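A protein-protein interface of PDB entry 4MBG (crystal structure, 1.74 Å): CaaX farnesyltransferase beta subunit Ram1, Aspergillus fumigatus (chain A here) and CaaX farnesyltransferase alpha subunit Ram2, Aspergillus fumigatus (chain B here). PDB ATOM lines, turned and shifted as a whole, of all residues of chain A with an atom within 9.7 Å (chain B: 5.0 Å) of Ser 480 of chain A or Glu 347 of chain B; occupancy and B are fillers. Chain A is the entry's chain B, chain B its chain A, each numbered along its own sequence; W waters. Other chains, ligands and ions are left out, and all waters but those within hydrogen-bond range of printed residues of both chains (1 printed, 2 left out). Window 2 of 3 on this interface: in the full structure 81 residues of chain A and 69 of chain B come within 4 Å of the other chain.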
ATOM      1  N   PRO A  73     -13.223  10.961 -13.980  1.00  0.00           N
ATOM      2  CA  PRO A  73     -13.111  12.135 -14.858  1.00  0.00           C
ATOM      3  C   PRO A  73     -12.913  11.739 -16.311  1.00  0.00           C
ATOM      4  O   PRO A  73     -12.301  10.707 -16.582  1.00  0.00           O
ATOM      5  CB  PRO A  73     -11.838  12.840 -14.366  1.00  0.00           C
ATOM      6  CG  PRO A  73     -11.627  12.342 -12.991  1.00  0.00           C
ATOM      7  CD  PRO A  73     -12.163  10.942 -12.957  1.00  0.00           C
ATOM      8  N   LEU A  75     -10.869  12.712 -18.344  1.00  0.00           N
ATOM      9  CA  LEU A  75      -9.433  12.575 -18.656  1.00  0.00           C
ATOM     10  C   LEU A  75      -8.995  11.108 -18.702  1.00  0.00           C
ATOM     11  O   LEU A  75      -8.085  10.727 -19.457  1.00  0.00           O
ATOM     12  CB  LEU A  75      -8.593  13.339 -17.615  1.00  0.00           C
ATOM     13  CG  LEU A  75      -7.069  13.313 -17.787  1.00  0.00           C
ATOM     14  CD1 LEU A  75      -6.677  14.061 -19.087  1.00  0.00           C
ATOM     15  CD2 LEU A  75      -6.377  13.936 -16.544  1.00  0.00           C
ATOM     16  N   PHE A  76      -9.661  10.276 -17.913  1.00  0.00           N
ATOM     17  CA  PHE A  76      -9.297   8.862 -17.844  1.00  0.00           C
ATOM     18  C   PHE A  76     -10.225   7.952 -18.647  1.00  0.00           C
ATOM     19  O   PHE A  76     -10.147   6.726 -18.532  1.00  0.00           O
ATOM     20  CB  PHE A  76      -9.233   8.427 -16.374  1.00  0.00           C
ATOM     21  CG  PHE A  76      -8.245   9.213 -15.584  1.00  0.00           C
ATOM     22  CD1 PHE A  76      -6.878   9.000 -15.767  1.00  0.00           C
ATOM     23  CD2 PHE A  76      -8.662  10.214 -14.705  1.00  0.00           C
ATOM     24  CE1 PHE A  76      -5.956   9.741 -15.063  1.00  0.00           C
ATOM     25  CE2 PHE A  76      -7.731  10.972 -13.990  1.00  0.00           C
ATOM     26  CZ  PHE A  76      -6.388  10.739 -14.163  1.00  0.00           C
ATOM     27  N   TYR A 119     -14.315   7.026  -6.291  1.00  0.00           N
ATOM     28  CA  TYR A 119     -13.642   7.537  -7.486  1.00  0.00           C
ATOM     29  C   TYR A 119     -13.745   6.541  -8.638  1.00  0.00           C
ATOM     30  O   TYR A 119     -13.152   6.746  -9.702  1.00  0.00           O
ATOM     31  CB  TYR A 119     -12.170   7.805  -7.175  1.00  0.00           C
ATOM     32  CG  TYR A 119     -11.935   9.025  -6.304  1.00  0.00           C
ATOM     33  CD1 TYR A 119     -12.017  10.313  -6.837  1.00  0.00           C
ATOM     34  CD2 TYR A 119     -11.644   8.891  -4.944  1.00  0.00           C
ATOM     35  CE1 TYR A 119     -11.796  11.434  -6.049  1.00  0.00           C
ATOM     36  CE2 TYR A 119     -11.434  10.023  -4.139  1.00  0.00           C
ATOM     37  CZ  TYR A 119     -11.519  11.280  -4.698  1.00  0.00           C
ATOM     38  OH  TYR A 119     -11.281  12.389  -3.918  1.00  0.00           O
ATOM     39  N   SER A 346       8.200  14.805 -15.752  1.00  0.00           N
ATOM     40  CA  SER A 346       6.774  15.076 -15.872  1.00  0.00           C
ATOM     41  C   SER A 346       6.161  14.404 -17.100  1.00  0.00           C
ATOM     42  O   SER A 346       5.067  13.827 -17.027  1.00  0.00           O
ATOM     43  CB  SER A 346       6.547  16.608 -15.884  1.00  0.00           C
ATOM     44  OG  SER A 346       5.199  16.918 -16.194  1.00  0.00           O
ATOM     45  N   GLN A 349       4.410  10.637 -17.681  1.00  0.00           N
ATOM     46  CA  GLN A 349       3.048  10.231 -17.350  1.00  0.00           C
ATOM     47  C   GLN A 349       2.073  10.535 -18.478  1.00  0.00           C
ATOM     48  O   GLN A 349       2.095  11.644 -19.017  1.00  0.00           O
ATOM     49  CB  GLN A 349       2.598  10.952 -16.071  1.00  0.00           C
ATOM     50  CG  GLN A 349       1.365  10.304 -15.476  1.00  0.00           C
ATOM     51  CD  GLN A 349       1.065  10.820 -14.098  1.00  0.00           C
ATOM     52  OE1 GLN A 349       1.509  11.912 -13.729  1.00  0.00           O
ATOM     53  NE2 GLN A 349       0.278  10.055 -13.333  1.00  0.00           N
ATOM     54  N   VAL A 397       6.938  22.375  -2.723  1.00  0.00           N
ATOM     55  CA  VAL A 397       6.464  22.431  -4.097  1.00  0.00           C
ATOM     56  C   VAL A 397       5.314  21.459  -4.310  1.00  0.00           C
ATOM     57  O   VAL A 397       4.593  21.556  -5.307  1.00  0.00           O
ATOM     58  CB  VAL A 397       7.599  22.151  -5.126  1.00  0.00           C
ATOM     59  CG1 VAL A 397       8.689  23.208  -4.987  1.00  0.00           C
ATOM     60  CG2 VAL A 397       8.186  20.738  -4.941  1.00  0.00           C
ATOM     61  N   GLY A 398       5.145  20.525  -3.375  1.00  0.00           N
ATOM     62  CA  GLY A 398       4.074  19.544  -3.461  1.00  0.00           C
ATOM     63  C   GLY A 398       4.433  18.462  -4.473  1.00  0.00           C
ATOM     64  O   GLY A 398       5.585  18.317  -4.862  1.00  0.00           O
ATOM     65  N   ASN A 399       3.432  17.708  -4.902  1.00  0.00           N
ATOM     66  CA  ASN A 399       3.596  16.674  -5.912  1.00  0.00           C
ATOM     67  C   ASN A 399       3.442  17.248  -7.288  1.00  0.00           C
ATOM     68  O   ASN A 399       2.433  17.887  -7.585  1.00  0.00           O
ATOM     69  CB  ASN A 399       2.553  15.591  -5.684  1.00  0.00           C
ATOM     70  CG  ASN A 399       2.740  14.917  -4.359  1.00  0.00           C
ATOM     71  OD1 ASN A 399       3.833  14.439  -4.063  1.00  0.00           O
ATOM     72  ND2 ASN A 399       1.700  14.920  -3.525  1.00  0.00           N
ATOM     73  N   LEU A 400       4.437  17.014  -8.140  1.00  0.00           N
ATOM     74  CA  LEU A 400       4.463  17.648  -9.446  1.00  0.00           C
ATOM     75  C   LEU A 400       3.999  16.711 -10.568  1.00  0.00           C
ATOM     76  O   LEU A 400       4.194  17.002 -11.741  1.00  0.00           O
ATOM     77  CB  LEU A 400       5.868  18.175  -9.727  1.00  0.00           C
ATOM     78  CG  LEU A 400       6.360  19.238  -8.749  1.00  0.00           C
ATOM     79  CD1 LEU A 400       7.796  19.650  -9.128  1.00  0.00           C
ATOM     80  CD2 LEU A 400       5.452  20.454  -8.787  1.00  0.00           C
ATOM     81  N   TYR A 401       3.409  15.588 -10.183  1.00  0.00           N
ATOM     82  CA  TYR A 401       2.821  14.603 -11.095  1.00  0.00           C
ATOM     83  C   TYR A 401       1.387  14.308 -10.586  1.00  0.00           C
ATOM     84  O   TYR A 401       0.964  14.859  -9.567  1.00  0.00           O
ATOM     85  CB  TYR A 401       3.663  13.313 -11.117  1.00  0.00           C
ATOM     86  CG  TYR A 401       3.617  12.537  -9.820  1.00  0.00           C
ATOM     87  CD1 TYR A 401       4.368  12.944  -8.730  1.00  0.00           C
ATOM     88  CD2 TYR A 401       2.824  11.384  -9.696  1.00  0.00           C
ATOM     89  CE1 TYR A 401       4.321  12.253  -7.524  1.00  0.00           C
ATOM     90  CE2 TYR A 401       2.771  10.672  -8.480  1.00  0.00           C
ATOM     91  CZ  TYR A 401       3.539  11.107  -7.411  1.00  0.00           C
ATOM     92  OH  TYR A 401       3.507  10.428  -6.211  1.00  0.00           O
ATOM     93  N   SER A 402       0.646  13.449 -11.288  1.00  0.00           N
ATOM     94  CA  SER A 402      -0.723  13.132 -10.910  1.00  0.00           C
ATOM     95  C   SER A 402      -0.793  11.854 -10.095  1.00  0.00           C
ATOM     96  O   SER A 402      -0.648  10.750 -10.640  1.00  0.00           O
ATOM     97  CB  SER A 402      -1.626  13.021 -12.151  1.00  0.00           C
ATOM     98  OG  SER A 402      -2.915  12.534 -11.787  1.00  0.00           O
ATOM     99  N   ARG A 403      -0.984  11.982  -8.781  1.00  0.00           N
ATOM    100  CA  ARG A 403      -1.150  10.777  -7.948  1.00  0.00           C
ATOM    101  C   ARG A 403      -2.415  10.035  -8.353  1.00  0.00           C
ATOM    102  O   ARG A 403      -2.472   8.800  -8.338  1.00  0.00           O
ATOM    103  CB  ARG A 403      -1.196  11.147  -6.446  1.00  0.00           C
ATOM    104  CG  ARG A 403       0.172  11.622  -5.904  1.00  0.00           C
ATOM    105  CD  ARG A 403       0.145  11.776  -4.350  1.00  0.00           C
ATOM    106  NE  ARG A 403      -0.834  12.751  -3.942  1.00  0.00           N
ATOM    107  CZ  ARG A 403      -1.771  12.561  -3.022  1.00  0.00           C
ATOM    108  NH1 ARG A 403      -1.896  11.392  -2.377  1.00  0.00           N
ATOM    109  NH2 ARG A 403      -2.588  13.559  -2.760  1.00  0.00           N
ATOM    110  N   GLU A 404      -3.429  10.798  -8.733  1.00  0.00           N
ATOM    111  CA  GLU A 404      -4.685  10.186  -9.172  1.00  0.00           C
ATOM    112  C   GLU A 404      -4.445   9.276 -10.388  1.00  0.00           C
ATOM    113  O   GLU A 404      -4.883   8.128 -10.413  1.00  0.00           O
ATOM    114  CB  GLU A 404      -5.732  11.255  -9.518  1.00  0.00           C
ATOM    115  CG  GLU A 404      -6.961  10.614 -10.191  1.00  0.00           C
ATOM    116  CD  GLU A 404      -8.109  11.583 -10.451  1.00  0.00           C
ATOM    117  OE1 GLU A 404      -7.926  12.821 -10.327  1.00  0.00           O
ATOM    118  OE2 GLU A 404      -9.202  11.090 -10.781  1.00  0.00           O
ATOM    119  N   GLY A 405      -3.770   9.797 -11.406  1.00  0.00           N
ATOM    120  CA  GLY A 405      -3.515   8.990 -12.599  1.00  0.00           C
ATOM    121  C   GLY A 405      -2.739   7.713 -12.281  1.00  0.00           C
ATOM    122  O   GLY A 405      -3.079   6.617 -12.748  1.00  0.00           O
ATOM    123  N   LEU A 406      -1.679   7.842 -11.498  1.00  0.00           N
ATOM    124  CA  LEU A 406      -0.873   6.668 -11.195  1.00  0.00           C
ATOM    125  C   LEU A 406      -1.684   5.622 -10.422  1.00  0.00           C
ATOM    126  O   LEU A 406      -1.594   4.410 -10.676  1.00  0.00           O
ATOM    127  CB  LEU A 406       0.371   7.064 -10.400  1.00  0.00           C
ATOM    128  CG  LEU A 406       1.304   5.888 -10.121  1.00  0.00           C
ATOM    129  CD1 LEU A 406       1.830   5.303 -11.429  1.00  0.00           C
ATOM    130  CD2 LEU A 406       2.455   6.326  -9.207  1.00  0.00           C
ATOM    131  N   SER A 475      -8.362  11.106  -0.135  1.00  0.00           N
ATOM    132  CA  SER A 475      -9.028  12.388  -0.354  1.00  0.00           C
ATOM    133  C   SER A 475     -10.526  12.229  -0.533  1.00  0.00           C
ATOM    134  O   SER A 475     -11.038  11.118  -0.679  1.00  0.00           O
ATOM    135  CB  SER A 475      -8.438  13.074  -1.613  1.00  0.00           C
ATOM    136  OG  SER A 475      -7.039  13.285  -1.480  1.00  0.00           O
ATOM    137  N   ASP A 476     -11.220  13.359  -0.499  1.00  0.00           N
ATOM    138  CA  ASP A 476     -12.623  13.433  -0.882  1.00  0.00           C
ATOM    139  C   ASP A 476     -12.750  14.564  -1.913  1.00  0.00           C
ATOM    140  O   ASP A 476     -12.070  15.579  -1.813  1.00  0.00           O
ATOM    141  CB  ASP A 476     -13.491  13.688   0.364  1.00  0.00           C
ATOM    142  CG  ASP A 476     -14.975  13.587   0.072  1.00  0.00           C
ATOM    143  OD1 ASP A 476     -15.439  12.495  -0.317  1.00  0.00           O
ATOM    144  OD2 ASP A 476     -15.682  14.595   0.252  1.00  0.00           O
ATOM    145  N   GLY A 477     -13.584  14.386  -2.927  1.00  0.00           N
ATOM    146  CA  GLY A 477     -13.775  15.441  -3.907  1.00  0.00           C
ATOM    147  C   GLY A 477     -12.726  15.505  -5.006  1.00  0.00           C
ATOM    148  O   GLY A 477     -11.775  14.726  -5.033  1.00  0.00           O
ATOM    149  N   GLN A 478     -12.902  16.458  -5.913  1.00  0.00           N
ATOM    150  CA  GLN A 478     -12.015  16.612  -7.054  1.00  0.00           C
ATOM    151  C   GLN A 478     -10.815  17.473  -6.668  1.00  0.00           C
ATOM    152  O   GLN A 478     -10.835  18.170  -5.663  1.00  0.00           O
ATOM    153  CB  GLN A 478     -12.776  17.238  -8.230  1.00  0.00           C
ATOM    154  CG  GLN A 478     -13.664  16.263  -9.007  1.00  0.00           C
ATOM    155  CD  GLN A 478     -14.089  16.813 -10.365  1.00  0.00           C
ATOM    156  OE1 GLN A 478     -14.838  17.787 -10.445  1.00  0.00           O
ATOM    157  NE2 GLN A 478     -13.603  16.193 -11.438  1.00  0.00           N
ATOM    158  N   GLY A 479      -9.756  17.429  -7.461  1.00  0.00           N
ATOM    159  CA  GLY A 479      -8.592  18.233  -7.148  1.00  0.00           C
ATOM    160  C   GLY A 479      -7.417  17.787  -7.982  1.00  0.00           C
ATOM    161  O   GLY A 479      -7.441  16.697  -8.534  1.00  0.00           O
ATOM    162  N   SER A 480      -6.389  18.624  -8.070  1.00  0.00           N
ATOM    163  CA  SER A 480      -5.222  18.305  -8.908  1.00  0.00           C
ATOM    164  C   SER A 480      -4.237  17.374  -8.225  1.00  0.00           C
ATOM    165  O   SER A 480      -3.417  16.745  -8.886  1.00  0.00           O
ATOM    166  CB  SER A 480      -4.501  19.586  -9.324  1.00  0.00           C
ATOM    167  OG  SER A 480      -3.673  20.079  -8.295  1.00  0.00           O
ATOM    168  N   ASP A 481      -4.306  17.290  -6.899  1.00  0.00           N
ATOM    169  CA  ASP A 481      -3.342  16.484  -6.157  1.00  0.00           C
ATOM    170  C   ASP A 481      -4.064  15.727  -5.065  1.00  0.00           C
ATOM    171  O   ASP A 481      -4.078  16.158  -3.911  1.00  0.00           O
ATOM    172  CB  ASP A 481      -2.242  17.368  -5.566  1.00  0.00           C
ATOM    173  CG  ASP A 481      -1.195  16.563  -4.806  1.00  0.00           C
ATOM    174  OD1 ASP A 481      -1.012  15.354  -5.099  1.00  0.00           O
ATOM    175  OD2 ASP A 481      -0.558  17.137  -3.911  1.00  0.00           O
ATOM    176  N   ILE A 482      -4.654  14.591  -5.439  1.00  0.00           N
ATOM    177  CA  ILE A 482      -5.559  13.877  -4.551  1.00  0.00           C
ATOM    178  C   ILE A 482      -5.227  12.402  -4.424  1.00  0.00           C
ATOM    179  O   ILE A 482      -4.593  11.787  -5.313  1.00  0.00           O
ATOM    180  CB  ILE A 482      -7.055  14.027  -4.984  1.00  0.00           C
ATOM    181  CG1 ILE A 482      -7.247  13.579  -6.446  1.00  0.00           C
ATOM    182  CG2 ILE A 482      -7.551  15.464  -4.727  1.00  0.00           C
ATOM    183  CD1 ILE A 482      -8.737  13.466  -6.890  1.00  0.00           C
ATOM    184  N   GLY A 483      -5.655  11.843  -3.302  1.00  0.00           N
ATOM    185  CA  GLY A 483      -5.432  10.433  -3.018  1.00  0.00           C
ATOM    186  C   GLY A 483      -6.708   9.679  -3.311  1.00  0.00           C
ATOM    187  O   GLY A 483      -7.671   9.758  -2.539  1.00  0.00           O
ATOM    188  N   VAL A 484      -6.720   8.930  -4.414  1.00  0.00           N
ATOM    189  CA  VAL A 484      -7.950   8.262  -4.860  1.00  0.00           C
ATOM    190  C   VAL A 484      -7.974   6.768  -4.525  1.00  0.00           C
ATOM    191  O   VAL A 484      -8.932   6.071  -4.853  1.00  0.00           O
ATOM    192  CB  VAL A 484      -8.211   8.477  -6.374  1.00  0.00           C
ATOM    193  CG1 VAL A 484      -8.331   9.952  -6.674  1.00  0.00           C
ATOM    194  CG2 VAL A 484      -7.066   7.873  -7.217  1.00  0.00           C
ATOM    195  N   LYS B 335      -2.736  22.689 -19.045  1.00  0.00           N
ATOM    196  CA  LYS B 335      -3.318  22.041 -17.876  1.00  0.00           C
ATOM    197  C   LYS B 335      -4.804  21.712 -18.036  1.00  0.00           C
ATOM    198  O   LYS B 335      -5.283  20.739 -17.454  1.00  0.00           O
ATOM    199  CB  LYS B 335      -3.046  22.844 -16.593  1.00  0.00           C
ATOM    200  CG  LYS B 335      -3.897  24.027 -16.409  1.00  0.00           C
ATOM    201  CD  LYS B 335      -3.544  24.724 -15.074  1.00  0.00           C
ATOM    202  CE  LYS B 335      -4.633  25.694 -14.715  1.00  0.00           C
ATOM    203  NZ  LYS B 335      -4.359  26.320 -13.419  1.00  0.00           N
ATOM    204  N   ARG B 343      -0.826  18.560 -15.072  1.00  0.00           N
ATOM    205  CA  ARG B 343      -1.331  19.804 -14.473  1.00  0.00           C
ATOM    206  C   ARG B 343      -0.468  20.350 -13.323  1.00  0.00           C
ATOM    207  O   ARG B 343      -0.230  21.570 -13.228  1.00  0.00           O
ATOM    208  CB  ARG B 343      -2.776  19.625 -13.993  1.00  0.00           C
ATOM    209  CG  ARG B 343      -3.342  20.877 -13.334  1.00  0.00           C
ATOM    210  CD  ARG B 343      -4.863  20.816 -13.140  1.00  0.00           C
ATOM    211  NE  ARG B 343      -5.364  22.133 -12.751  1.00  0.00           N
ATOM    212  CZ  ARG B 343      -6.407  22.741 -13.307  1.00  0.00           C
ATOM    213  NH1 ARG B 343      -7.094  22.154 -14.280  1.00  0.00           N
ATOM    214  NH2 ARG B 343      -6.765  23.938 -12.884  1.00  0.00           N
ATOM    215  N   ASN B 344       0.013  19.476 -12.451  1.00  0.00           N
ATOM    216  CA  ASN B 344       0.797  19.959 -11.302  1.00  0.00           C
ATOM    217  C   ASN B 344       2.139  20.542 -11.717  1.00  0.00           C
ATOM    218  O   ASN B 344       2.622  21.490 -11.103  1.00  0.00           O
ATOM    219  CB  ASN B 344       0.955  18.881 -10.221  1.00  0.00           C
ATOM    220  CG  ASN B 344      -0.346  18.583  -9.527  1.00  0.00           C
ATOM    221  OD1 ASN B 344      -1.161  19.491  -9.303  1.00  0.00           O
ATOM    222  ND2 ASN B 344      -0.574  17.325  -9.210  1.00  0.00           N
ATOM    223  N   TYR B 345       2.727  19.982 -12.772  1.00  0.00           N
ATOM    224  CA  TYR B 345       3.945  20.566 -13.335  1.00  0.00           C
ATOM    225  C   TYR B 345       3.646  21.919 -14.022  1.00  0.00           C
ATOM    226  O   TYR B 345       4.358  22.915 -13.809  1.00  0.00           O
ATOM    227  CB  TYR B 345       4.633  19.581 -14.305  1.00  0.00           C
ATOM    228  CG  TYR B 345       5.794  20.244 -15.002  1.00  0.00           C
ATOM    229  CD1 TYR B 345       6.928  20.654 -14.284  1.00  0.00           C
ATOM    230  CD2 TYR B 345       5.743  20.511 -16.363  1.00  0.00           C
ATOM    231  CE1 TYR B 345       7.983  21.309 -14.925  1.00  0.00           C
ATOM    232  CE2 TYR B 345       6.802  21.157 -17.003  1.00  0.00           C
ATOM    233  CZ  TYR B 345       7.889  21.566 -16.279  1.00  0.00           C
ATOM    234  OH  TYR B 345       8.903  22.214 -16.939  1.00  0.00           O
ATOM    235  N   TRP B 346       2.589  21.972 -14.834  1.00  0.00           N
ATOM    236  CA  TRP B 346       2.223  23.247 -15.448  1.00  0.00           C
ATOM    237  C   TRP B 346       1.948  24.329 -14.389  1.00  0.00           C
ATOM    238  O   TRP B 346       2.352  25.494 -14.566  1.00  0.00           O
ATOM    239  CB  TRP B 346       1.007  23.101 -16.368  1.00  0.00           C
ATOM    240  CG  TRP B 346       1.110  21.974 -17.423  1.00  0.00           C
ATOM    241  CD1 TRP B 346       0.160  21.047 -17.687  1.00  0.00           C
ATOM    242  CD2 TRP B 346       2.205  21.694 -18.318  1.00  0.00           C
ATOM    243  NE1 TRP B 346       0.572  20.204 -18.691  1.00  0.00           N
ATOM    244  CE2 TRP B 346       1.821  20.577 -19.106  1.00  0.00           C
ATOM    245  CE3 TRP B 346       3.456  22.280 -18.546  1.00  0.00           C
ATOM    246  CZ2 TRP B 346       2.654  20.012 -20.090  1.00  0.00           C
ATOM    247  CZ3 TRP B 346       4.292  21.720 -19.528  1.00  0.00           C
ATOM    248  CH2 TRP B 346       3.882  20.599 -20.288  1.00  0.00           C
ATOM    249  N   GLU B 347       1.269  23.949 -13.303  1.00  0.00           N
ATOM    250  CA  GLU B 347       0.949  24.884 -12.225  1.00  0.00           C
ATOM    251  C   GLU B 347       2.223  25.340 -11.499  1.00  0.00           C
ATOM    252  O   GLU B 347       2.344  26.492 -11.086  1.00  0.00           O
ATOM    253  CB  GLU B 347      -0.122  24.295 -11.268  1.00  0.00           C
ATOM    254  CG  GLU B 347      -1.547  24.262 -11.897  1.00  0.00           C
ATOM    255  CD  GLU B 347      -2.676  23.725 -10.988  1.00  0.00           C
ATOM    256  OE1 GLU B 347      -2.408  23.196  -9.890  1.00  0.00           O
ATOM    257  OE2 GLU B 347      -3.856  23.828 -11.390  1.00  0.00           O
ATOM    258  N   TYR B 348       3.185  24.436 -11.360  1.00  0.00           N
ATOM    259  CA  TYR B 348       4.484  24.811 -10.808  1.00  0.00           C
ATOM    260  C   TYR B 348       5.152  25.869 -11.702  1.00  0.00           C
ATOM    261  O   TYR B 348       5.708  26.865 -11.209  1.00  0.00           O
ATOM    262  CB  TYR B 348       5.364  23.577 -10.673  1.00  0.00           C
ATOM    263  CG  TYR B 348       6.797  23.844 -10.284  1.00  0.00           C
ATOM    264  CD1 TYR B 348       7.126  24.186  -8.976  1.00  0.00           C
ATOM    265  CD2 TYR B 348       7.821  23.746 -11.220  1.00  0.00           C
ATOM    266  CE1 TYR B 348       8.445  24.404  -8.602  1.00  0.00           C
ATOM    267  CE2 TYR B 348       9.134  23.968 -10.859  1.00  0.00           C
ATOM    268  CZ  TYR B 348       9.439  24.302  -9.548  1.00  0.00           C
ATOM    269  OH  TYR B 348      10.739  24.530  -9.179  1.00  0.00           O
ATOM    270  N   ARG B 349       5.080  25.665 -13.011  1.00  0.00           N
ATOM    271  CA  ARG B 349       5.646  26.641 -13.949  1.00  0.00           C
ATOM    272  C   ARG B 349       4.914  27.976 -13.819  1.00  0.00           C
ATOM    273  O   ARG B 349       5.540  29.036 -13.772  1.00  0.00           O
ATOM    274  CB  ARG B 349       5.608  26.131 -15.402  1.00  0.00           C
ATOM    275  CG  ARG B 349       6.595  24.978 -15.665  1.00  0.00           C
ATOM    276  CD  ARG B 349       8.057  25.494 -15.671  1.00  0.00           C
ATOM    277  NE  ARG B 349       8.323  26.346 -16.835  1.00  0.00           N
ATOM    278  CZ  ARG B 349       8.935  27.525 -16.780  1.00  0.00           C
ATOM    279  NH1 ARG B 349       9.356  28.005 -15.618  1.00  0.00           N
ATOM    280  NH2 ARG B 349       9.136  28.224 -17.890  1.00  0.00           N
ATOM    281  N   ILE B 350       3.591  27.924 -13.739  1.00  0.00           N
ATOM    282  CA  ILE B 350       2.813  29.167 -13.564  1.00  0.00           C
ATOM    283  C   ILE B 350       3.246  29.896 -12.294  1.00  0.00           C
ATOM    284  O   ILE B 350       3.430  31.124 -12.299  1.00  0.00           O
ATOM    285  CB  ILE B 350       1.300  28.897 -13.542  1.00  0.00           C
ATOM    286  CG1 ILE B 350       0.833  28.463 -14.941  1.00  0.00           C
ATOM    287  CG2 ILE B 350       0.549  30.141 -13.081  1.00  0.00           C
ATOM    288  CD1 ILE B 350      -0.602  27.893 -15.011  1.00  0.00           C
ATOM    289  N   ARG B 351       3.451  29.159 -11.211  1.00  0.00           N
ATOM    290  CA  ARG B 351       3.901  29.768  -9.954  1.00  0.00           C
ATOM    291  C   ARG B 351       5.276  30.414 -10.102  1.00  0.00           C
ATOM    292  O   ARG B 351       5.513  31.505  -9.592  1.00  0.00           O
ATOM    293  CB  ARG B 351       3.925  28.743  -8.811  1.00  0.00           C
ATOM    294  CG  ARG B 351       2.547  28.251  -8.389  1.00  0.00           C
ATOM    295  CD  ARG B 351       2.552  27.604  -6.994  1.00  0.00           C
ATOM    296  NE  ARG B 351       3.408  26.423  -6.879  1.00  0.00           N
ATOM    297  CZ  ARG B 351       3.047  25.187  -7.224  1.00  0.00           C
ATOM    298  NH1 ARG B 351       1.852  24.969  -7.744  1.00  0.00           N
ATOM    299  NH2 ARG B 351       3.891  24.167  -7.063  1.00  0.00           N
HETATM  300  O   HOH W   1      -2.868  16.507 -11.550  1.00  0.00           O
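O of Asn 399 of chain A sits close to ND2 of Asn 344 of chain B (3.5 Å). ND2 of Asn 344 of chain B lies within hydrogen-bond range of O of Tyr 401 of chain A (2.9 Å). The side-chain amide oxygen (OD1) of Asn 344 of chain B lies within hydrogen-bond range of the side-chain hydroxyl (OG) of Ser 480 of chain A (2.8 Å). N of Tyr 345 of chain B sits at hydrogen-bond distance from O of Leu 400 of chain A, at 3.5 Å. The backbone carbonyl oxygen (O) of Val 397 of chain A sits at hydrogen-bond distance from the guanidinium group (NH2) of Arg 351 of chain B (3.2 Å).
NZ of Lys 335 of chain B is in salt-bridge range of OE2 of Glu 347 of chain B (3.3 Å). The side-chain carboxylate (OE2) of Glu 347 of chain B lies within salt-bridge range of the guanidinium group (NE) of Arg 343 of chain B (2.6 Å). NE of Arg 403 of chain A lies close to ND2 of Asn 399 of chain A (3.4 Å). ND2 of Asn 399 of chain A sits at hydrogen-bond distance from OD1 of Asp 481 of chain A, 3.2 Å away.
Among the printed residues, merely in contact across the chains: Ser 346 of chain A with Tyr 345 of chain B (3.3 Å), Val 397 of chain A with Tyr 348 of chain B (3.8 Å), Leu 400 of chain A with Asn 344 of chain B (3.8 Å), Leu 400 of chain A with Tyr 348 of chain B (3.6 Å) and Ser 480 of chain A with Glu 347 of chain B (3.7 Å).
Printed residues of chain B within 4 Å of Ser 480 of chain A: Asn 344 (2.8 Å) and Glu 347 (3.7 Å). Of the printed residues of chain A, Glu 347 of chain B touches Ser 480. Printed residues of chain A within 4 Å of Arg 351 of chain B: Val 397 (3.2 Å). Printed residues of chain B within 4 Å of Val 397 of chain A: Tyr 348 (3.8 Å) and Arg 351 (3.2 Å). Gln 349 of chain A touches none of the printed residues of chain B. Val 484 of chain A touches none of the printed residues of chain B. The nearest printed residue of chain A that does not touch Glu 347 of chain B is Leu 400 of chain A (6.5 Å).
Of the 10 printed residues of chain B, 5 touch a printed residue of chain A. Printed residues of chain B that touch a printed residue of chain A: Asn 344, Tyr 345, Glu 347, Tyr 348 and Arg 351. Of the 26 printed residues of chain A, 6 touch a printed residue of chain B. Hydrophobic or aromatic side chains of chain A that line the printed part of chain B: Val 397 and Leu 400. Among the printed residues, no Asp or Glu carboxylate lies within 4 Å of a Lys or Arg side-chain nitrogen of the other chain.
Water W1 bridges O of Ser 480 of chain A (2.7 Å) and ND2 of Asn 344 of chain B (3.4 Å).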
